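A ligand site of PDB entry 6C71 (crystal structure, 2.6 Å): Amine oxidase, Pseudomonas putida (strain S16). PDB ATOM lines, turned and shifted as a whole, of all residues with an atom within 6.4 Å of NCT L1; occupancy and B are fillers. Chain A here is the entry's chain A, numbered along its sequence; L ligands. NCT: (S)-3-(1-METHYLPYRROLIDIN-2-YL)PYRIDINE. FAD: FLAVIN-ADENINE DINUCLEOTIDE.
The side-chain hydroxyl (OG1) of Thr 381 sits at hydrogen-bond distance from a nitrogen (N1) of NCT L1 (2.9 Å).
A nitrogen (N2) of NCT L1 sits close to the side-chain hydroxyl (OH) of Tyr 218, at 3.4 Å.
N2 of NCT L1 is in salt-bridge range of OE2 of Glu 249 (3.7 Å).
An oxygen (O3') of FAD L2 is in hydrogen-bond range of the backbone carbonyl oxygen of Asn 462 (3.0 Å).
N of Trp 108 sits at hydrogen-bond distance from O4 of FAD L2 (3.1 Å).
The backbone carbonyl oxygen of Trp 108 sits at hydrogen-bond distance from a nitrogen (N3) of FAD L2 (2.8 Å).
N of Thr 381 is in hydrogen-bond range of O of Trp 364 (2.8 Å).
The indole nitrogen (NE1) of Trp 427 is in hydrogen-bond range of the backbone carbonyl oxygen (O) of Tyr 218 (3.2 Å).
The side-chain amide oxygen (OE1) of Gln 366 is in hydrogen-bond range of the indole nitrogen (NE1) of Trp 364 (3.2 Å).
NE1 of Trp 108 lies within hydrogen-bond range of O of Thr 250 (3.5 Å).
The side-chain hydroxyl (OG1) of Thr 250 sits close to the side-chain amide oxygen (OE1) of Gln 366 (3.3 Å).
O of Leu 217 sits close to NE1 of Trp 427 (3.1 Å).
Trp 108 touches NCT L1 (CZ3 to N1, 3.9 Å).
Leu 217 touches NCT L1 (CD1 to C3, 3.6 Å).
Thr 250 touches NCT L1.
Trp 364 touches NCT L1.
CD2 of Trp 427 touches C7 of NCT L1, 3.7 Å away.
O of Ala 461 touches C9 of NCT L1 (3.4 Å).
ND2 of Asn 462 touches C10 of NCT L1, 3.9 Å away.
Hydrophobic or aromatic side chains within 4 Å of NCT L1: Trp 108, Leu 217, Tyr 218, Trp 364, Trp 427 and Ala 461.
Within 4 Å of NCT L1: Trp 108, Leu 217, Tyr 218, Glu 249, Thr 250, Trp 364, Thr 381, Trp 427, Ala 461 and Asn 462.
The nearest printed residue that does not touch NCT L1 is Lys 340 (5.7 Å).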
ATOM      1  N   TRP A 108      -0.586  19.608   8.042  1.00  0.00           N
ATOM      2  CA  TRP A 108      -1.790  19.309   8.807  1.00  0.00           C
ATOM      3  C   TRP A 108      -2.979  20.147   8.325  1.00  0.00           C
ATOM      4  O   TRP A 108      -2.845  21.346   8.079  1.00  0.00           O
ATOM      5  CB  TRP A 108      -1.566  19.533  10.296  1.00  0.00           C
ATOM      6  CG  TRP A 108      -0.518  18.631  10.860  1.00  0.00           C
ATOM      7  CD1 TRP A 108      -0.607  17.279  11.025  1.00  0.00           C
ATOM      8  CD2 TRP A 108       0.790  18.999  11.312  1.00  0.00           C
ATOM      9  NE1 TRP A 108       0.560  16.792  11.558  1.00  0.00           N
ATOM     10  CE2 TRP A 108       1.429  17.830  11.748  1.00  0.00           C
ATOM     11  CE3 TRP A 108       1.481  20.212  11.396  1.00  0.00           C
ATOM     12  CZ2 TRP A 108       2.733  17.827  12.256  1.00  0.00           C
ATOM     13  CZ3 TRP A 108       2.766  20.222  11.905  1.00  0.00           C
ATOM     14  CH2 TRP A 108       3.383  19.037  12.326  1.00  0.00           C
ATOM     15  N   TYR A 214       4.343  29.286  21.454  1.00  0.00           N
ATOM     16  CA  TYR A 214       3.320  29.144  20.420  1.00  0.00           C
ATOM     17  C   TYR A 214       3.342  30.331  19.471  1.00  0.00           C
ATOM     18  O   TYR A 214       3.460  30.167  18.247  1.00  0.00           O
ATOM     19  CB  TYR A 214       1.953  28.984  21.092  1.00  0.00           C
ATOM     20  CG  TYR A 214       0.894  28.246  20.321  1.00  0.00           C
ATOM     21  CD1 TYR A 214       0.202  27.189  20.904  1.00  0.00           C
ATOM     22  CD2 TYR A 214       0.578  28.589  19.015  1.00  0.00           C
ATOM     23  CE1 TYR A 214      -0.773  26.499  20.198  1.00  0.00           C
ATOM     24  CE2 TYR A 214      -0.396  27.908  18.312  1.00  0.00           C
ATOM     25  CZ  TYR A 214      -1.067  26.857  18.907  1.00  0.00           C
ATOM     26  OH  TYR A 214      -2.041  26.177  18.203  1.00  0.00           O
ATOM     27  N   LEU A 217       6.482  30.658  17.352  1.00  0.00           N
ATOM     28  CA  LEU A 217       6.482  29.751  16.203  1.00  0.00           C
ATOM     29  C   LEU A 217       5.555  30.258  15.114  1.00  0.00           C
ATOM     30  O   LEU A 217       5.910  30.247  13.923  1.00  0.00           O
ATOM     31  CB  LEU A 217       6.105  28.330  16.645  1.00  0.00           C
ATOM     32  CG  LEU A 217       6.141  27.161  15.648  1.00  0.00           C
ATOM     33  CD1 LEU A 217       5.035  27.171  14.569  1.00  0.00           C
ATOM     34  CD2 LEU A 217       7.498  27.146  14.980  1.00  0.00           C
ATOM     35  N   TYR A 218       4.361  30.742  15.478  1.00  0.00           N
ATOM     36  CA  TYR A 218       3.461  31.243  14.451  1.00  0.00           C
ATOM     37  C   TYR A 218       3.999  32.518  13.792  1.00  0.00           C
ATOM     38  O   TYR A 218       3.653  32.811  12.638  1.00  0.00           O
ATOM     39  CB  TYR A 218       2.072  31.484  15.041  1.00  0.00           C
ATOM     40  CG  TYR A 218       1.194  30.273  14.846  1.00  0.00           C
ATOM     41  CD1 TYR A 218       0.046  30.346  14.075  1.00  0.00           C
ATOM     42  CD2 TYR A 218       1.562  29.051  15.379  1.00  0.00           C
ATOM     43  CE1 TYR A 218      -0.741  29.228  13.883  1.00  0.00           C
ATOM     44  CE2 TYR A 218       0.785  27.932  15.188  1.00  0.00           C
ATOM     45  CZ  TYR A 218      -0.370  28.031  14.442  1.00  0.00           C
ATOM     46  OH  TYR A 218      -1.138  26.908  14.261  1.00  0.00           O
ATOM     47  N   GLU A 249      -4.559  22.389  14.003  1.00  0.00           N
ATOM     48  CA  GLU A 249      -3.245  22.857  13.597  1.00  0.00           C
ATOM     49  C   GLU A 249      -2.196  21.764  13.415  1.00  0.00           C
ATOM     50  O   GLU A 249      -1.394  21.847  12.473  1.00  0.00           O
ATOM     51  CB  GLU A 249      -2.731  23.897  14.586  1.00  0.00           C
ATOM     52  CG  GLU A 249      -3.619  25.123  14.640  1.00  0.00           C
ATOM     53  CD  GLU A 249      -3.799  25.761  13.280  1.00  0.00           C
ATOM     54  OE1 GLU A 249      -4.886  25.613  12.691  1.00  0.00           O
ATOM     55  OE2 GLU A 249      -2.853  26.420  12.791  1.00  0.00           O
ATOM     56  N   THR A 250      -2.137  20.741  14.280  1.00  0.00           N
ATOM     57  CA  THR A 250      -1.078  19.751  14.141  1.00  0.00           C
ATOM     58  C   THR A 250      -1.562  18.315  14.370  1.00  0.00           C
ATOM     59  O   THR A 250      -0.745  17.452  14.725  1.00  0.00           O
ATOM     60  CB  THR A 250       0.092  20.017  15.096  1.00  0.00           C
ATOM     61  OG1 THR A 250      -0.383  20.079  16.444  1.00  0.00           O
ATOM     62  CG2 THR A 250       0.815  21.310  14.738  1.00  0.00           C
ATOM     63  N   LYS A 340      11.989  23.241   9.253  1.00  0.00           N
ATOM     64  CA  LYS A 340      11.450  22.023   9.842  1.00  0.00           C
ATOM     65  C   LYS A 340      12.513  20.947   9.910  1.00  0.00           C
ATOM     66  O   LYS A 340      13.284  20.756   8.970  1.00  0.00           O
ATOM     67  CB  LYS A 340      10.215  21.515   9.089  1.00  0.00           C
ATOM     68  CG  LYS A 340       9.475  20.440   9.880  1.00  0.00           C
ATOM     69  CD  LYS A 340       7.975  20.479   9.686  1.00  0.00           C
ATOM     70  CE  LYS A 340       7.317  19.309  10.401  1.00  0.00           C
ATOM     71  NZ  LYS A 340       5.930  19.042   9.945  1.00  0.00           N
ATOM     72  N   TRP A 364       8.811  23.775  18.553  1.00  0.00           N
ATOM     73  CA  TRP A 364       7.636  22.912  18.517  1.00  0.00           C
ATOM     74  C   TRP A 364       8.070  21.469  18.313  1.00  0.00           C
ATOM     75  O   TRP A 364       8.595  21.124  17.256  1.00  0.00           O
ATOM     76  CB  TRP A 364       6.661  23.354  17.422  1.00  0.00           C
ATOM     77  CG  TRP A 364       5.304  22.695  17.490  1.00  0.00           C
ATOM     78  CD1 TRP A 364       5.019  21.384  17.275  1.00  0.00           C
ATOM     79  CD2 TRP A 364       4.049  23.332  17.792  1.00  0.00           C
ATOM     80  NE1 TRP A 364       3.670  21.159  17.423  1.00  0.00           N
ATOM     81  CE2 TRP A 364       3.051  22.341  17.738  1.00  0.00           C
ATOM     82  CE3 TRP A 364       3.688  24.653  18.097  1.00  0.00           C
ATOM     83  CZ2 TRP A 364       1.707  22.621  17.981  1.00  0.00           C
ATOM     84  CZ3 TRP A 364       2.353  24.921  18.338  1.00  0.00           C
ATOM     85  CH2 TRP A 364       1.384  23.919  18.274  1.00  0.00           C
ATOM     86  N   GLN A 366       6.871  17.312  18.605  1.00  0.00           N
ATOM     87  CA  GLN A 366       5.798  16.342  18.777  1.00  0.00           C
ATOM     88  C   GLN A 366       6.222  15.038  18.120  1.00  0.00           C
ATOM     89  O   GLN A 366       7.070  15.013  17.229  1.00  0.00           O
ATOM     90  CB  GLN A 366       4.461  16.835  18.205  1.00  0.00           C
ATOM     91  CG  GLN A 366       4.471  17.159  16.729  1.00  0.00           C
ATOM     92  CD  GLN A 366       3.079  17.452  16.205  1.00  0.00           C
ATOM     93  OE1 GLN A 366       2.405  18.361  16.675  1.00  0.00           O
ATOM     94  NE2 GLN A 366       2.633  16.648  15.237  1.00  0.00           N
ATOM     95  N   ILE A 380       9.769  18.374  14.509  1.00  0.00           N
ATOM     96  CA  ILE A 380      10.163  19.606  15.184  1.00  0.00           C
ATOM     97  C   ILE A 380      10.031  20.756  14.198  1.00  0.00           C
ATOM     98  O   ILE A 380      10.527  20.674  13.072  1.00  0.00           O
ATOM     99  CB  ILE A 380      11.598  19.529  15.734  1.00  0.00           C
ATOM    100  CG1 ILE A 380      11.773  18.285  16.610  1.00  0.00           C
ATOM    101  CG2 ILE A 380      11.951  20.786  16.504  1.00  0.00           C
ATOM    102  CD1 ILE A 380      13.150  18.160  17.219  1.00  0.00           C
ATOM    103  N   THR A 381       9.366  21.825  14.630  1.00  0.00           N
ATOM    104  CA  THR A 381       9.288  23.065  13.871  1.00  0.00           C
ATOM    105  C   THR A 381      10.064  24.140  14.605  1.00  0.00           C
ATOM    106  O   THR A 381       9.900  24.331  15.822  1.00  0.00           O
ATOM    107  CB  THR A 381       7.833  23.502  13.670  1.00  0.00           C
ATOM    108  OG1 THR A 381       7.023  22.340  13.407  1.00  0.00           O
ATOM    109  CG2 THR A 381       7.726  24.469  12.515  1.00  0.00           C
ATOM    110  N   TRP A 427       5.644  29.863   6.641  1.00  0.00           N
ATOM    111  CA  TRP A 427       4.225  30.207   6.566  1.00  0.00           C
ATOM    112  C   TRP A 427       4.035  31.725   6.635  1.00  0.00           C
ATOM    113  O   TRP A 427       4.892  32.470   7.090  1.00  0.00           O
ATOM    114  CB  TRP A 427       3.481  29.541   7.708  1.00  0.00           C
ATOM    115  CG  TRP A 427       4.237  29.689   8.995  1.00  0.00           C
ATOM    116  CD1 TRP A 427       4.144  30.698   9.905  1.00  0.00           C
ATOM    117  CD2 TRP A 427       5.270  28.815   9.482  1.00  0.00           C
ATOM    118  NE1 TRP A 427       5.029  30.506  10.934  1.00  0.00           N
ATOM    119  CE2 TRP A 427       5.729  29.349  10.701  1.00  0.00           C
ATOM    120  CE3 TRP A 427       5.832  27.621   9.008  1.00  0.00           C
ATOM    121  CZ2 TRP A 427       6.734  28.730  11.454  1.00  0.00           C
ATOM    122  CZ3 TRP A 427       6.828  27.013   9.763  1.00  0.00           C
ATOM    123  CH2 TRP A 427       7.260  27.574  10.966  1.00  0.00           C
ATOM    124  N   ALA A 428       2.852  32.190   6.209  1.00  0.00           N
ATOM    125  CA  ALA A 428       2.540  33.619   6.274  1.00  0.00           C
ATOM    126  C   ALA A 428       2.441  34.084   7.715  1.00  0.00           C
ATOM    127  O   ALA A 428       1.744  33.481   8.535  1.00  0.00           O
ATOM    128  CB  ALA A 428       1.238  33.928   5.533  1.00  0.00           C
ATOM    129  N   ALA A 461      -2.204  31.430   7.380  1.00  0.00           N
ATOM    130  CA  ALA A 461      -1.009  30.697   7.752  1.00  0.00           C
ATOM    131  C   ALA A 461      -1.088  29.220   7.390  1.00  0.00           C
ATOM    132  O   ALA A 461      -0.298  28.419   7.900  1.00  0.00           O
ATOM    133  CB  ALA A 461      -0.733  30.851   9.250  1.00  0.00           C
ATOM    134  N   ASN A 462      -2.022  28.839   6.516  1.00  0.00           N
ATOM    135  CA  ASN A 462      -2.348  27.437   6.310  1.00  0.00           C
ATOM    136  C   ASN A 462      -2.472  27.119   4.826  1.00  0.00           C
ATOM    137  O   ASN A 462      -2.446  28.008   3.969  1.00  0.00           O
ATOM    138  CB  ASN A 462      -3.632  27.050   7.042  1.00  0.00           C
ATOM    139  CG  ASN A 462      -3.538  27.277   8.536  1.00  0.00           C
ATOM    140  OD1 ASN A 462      -3.758  28.388   9.030  1.00  0.00           O
ATOM    141  ND2 ASN A 462      -3.217  26.222   9.275  1.00  0.00           N
HETATM  142  N1  NCT L   1       4.411  23.561  13.154  1.00  0.00           N
HETATM  143  C1  NCT L   1       3.925  24.356  12.230  1.00  0.00           C
HETATM  144  C2  NCT L   1       2.801  25.160  12.501  1.00  0.00           C
HETATM  145  C3  NCT L   1       2.205  25.113  13.748  1.00  0.00           C
HETATM  146  C4  NCT L   1       2.747  24.276  14.697  1.00  0.00           C
HETATM  147  C5  NCT L   1       3.865  23.497  14.360  1.00  0.00           C
HETATM  148  N2  NCT L   1       0.647  26.146  11.477  1.00  0.00           N
HETATM  149  C6  NCT L   1       2.235  26.094  11.396  1.00  0.00           C
HETATM  150  C7  NCT L   1       2.654  27.343  11.596  1.00  0.00           C
HETATM  151  C8  NCT L   1       1.579  28.192  11.050  1.00  0.00           C
HETATM  152  C9  NCT L   1       0.296  27.275  11.038  1.00  0.00           C
HETATM  153  C10 NCT L   1       0.200  25.326  10.823  1.00  0.00           C
HETATM  154  PA  FAD L   2       3.825  28.299  -2.134  1.00  0.00           P
HETATM  155  O1A FAD L   2       5.110  28.830  -1.609  1.00  0.00           O
HETATM  156  O2A FAD L   2       3.370  26.943  -1.519  1.00  0.00           O
HETATM  157  O5B FAD L   2       3.864  28.226  -3.742  1.00  0.00           O
HETATM  158  C5B FAD L   2       4.503  29.211  -4.537  1.00  0.00           C
HETATM  159  C4B FAD L   2       5.204  28.530  -5.705  1.00  0.00           C
HETATM  160  O4B FAD L   2       5.794  29.535  -6.478  1.00  0.00           O
HETATM  161  C3B FAD L   2       6.335  27.633  -5.207  1.00  0.00           C
HETATM  162  O3B FAD L   2       6.218  26.361  -5.835  1.00  0.00           O
HETATM  163  C2B FAD L   2       7.595  28.310  -5.696  1.00  0.00           C
HETATM  164  O2B FAD L   2       8.507  27.294  -6.073  1.00  0.00           O
HETATM  165  C1B FAD L   2       7.100  29.140  -6.880  1.00  0.00           C
HETATM  166  N9A FAD L   2       7.845  30.364  -7.262  1.00  0.00           N
HETATM  167  C8A FAD L   2       8.389  31.351  -6.476  1.00  0.00           C
HETATM  168  N7A FAD L   2       8.973  32.291  -7.273  1.00  0.00           N
HETATM  169  C5A FAD L   2       8.806  31.916  -8.566  1.00  0.00           C
HETATM  170  C6A FAD L   2       9.190  32.494  -9.787  1.00  0.00           C
HETATM  171  N6A FAD L   2       9.891  33.678  -9.862  1.00  0.00           N
HETATM  172  N1A FAD L   2       8.833  31.811 -10.939  1.00  0.00           N
HETATM  173  C2A FAD L   2       8.132  30.620 -10.926  1.00  0.00           C
HETATM  174  N3A FAD L   2       7.764  30.084  -9.717  1.00  0.00           N
HETATM  175  C4A FAD L   2       8.095  30.718  -8.566  1.00  0.00           C
HETATM  176  N1  FAD L   2      -0.102  25.089   6.392  1.00  0.00           N
HETATM  177  C2  FAD L   2      -1.064  24.178   6.817  1.00  0.00           C
HETATM  178  O2  FAD L   2      -2.221  24.252   6.383  1.00  0.00           O
HETATM  179  N3  FAD L   2      -0.764  23.168   7.738  1.00  0.00           N
HETATM  180  C4  FAD L   2       0.531  23.077   8.227  1.00  0.00           C
HETATM  181  O4  FAD L   2       0.850  22.201   9.044  1.00  0.00           O
HETATM  182  C4X FAD L   2       1.492  23.977   7.810  1.00  0.00           C
HETATM  183  N5  FAD L   2       2.783  23.861   8.324  1.00  0.00           N
HETATM  184  C5X FAD L   2       3.804  24.673   7.902  1.00  0.00           C
HETATM  185  C6  FAD L   2       5.099  24.273   8.204  1.00  0.00           C
HETATM  186  C7  FAD L   2       6.161  24.633   7.374  1.00  0.00           C
HETATM  187  C7M FAD L   2       7.547  24.167   7.749  1.00  0.00           C
HETATM  188  C8  FAD L   2       5.891  25.412   6.222  1.00  0.00           C
HETATM  189  C8M FAD L   2       6.967  25.860   5.257  1.00  0.00           C
HETATM  190  C9  FAD L   2       4.574  25.800   5.937  1.00  0.00           C
HETATM  191  C9A FAD L   2       3.534  25.450   6.760  1.00  0.00           C
HETATM  192  N10 FAD L   2       2.206  25.841   6.516  1.00  0.00           N
HETATM  193  C10 FAD L   2       1.181  24.988   6.888  1.00  0.00           C
HETATM  194  C1' FAD L   2       1.927  26.942   5.543  1.00  0.00           C
HETATM  195  C2' FAD L   2       1.702  26.467   4.124  1.00  0.00           C
HETATM  196  O2' FAD L   2       2.098  25.172   3.774  1.00  0.00           O
HETATM  197  C3' FAD L   2       1.515  27.549   3.050  1.00  0.00           C
HETATM  198  O3' FAD L   2       0.493  28.406   3.501  1.00  0.00           O
HETATM  199  C4' FAD L   2       0.975  27.069   1.715  1.00  0.00           C
HETATM  200  O4' FAD L   2       1.698  25.961   1.237  1.00  0.00           O
HETATM  201  C5' FAD L   2       1.039  28.276   0.793  1.00  0.00           C
HETATM  202  O5' FAD L   2       0.938  27.849  -0.528  1.00  0.00           O
HETATM  203  P   FAD L   2       1.057  28.937  -1.738  1.00  0.00           P
HETATM  204  O1P FAD L   2       0.556  28.361  -3.030  1.00  0.00           O
HETATM  205  O2P FAD L   2       0.175  30.132  -1.302  1.00  0.00           O
HETATM  206  O3P FAD L   2       2.481  29.285  -1.878  1.00  0.00           O
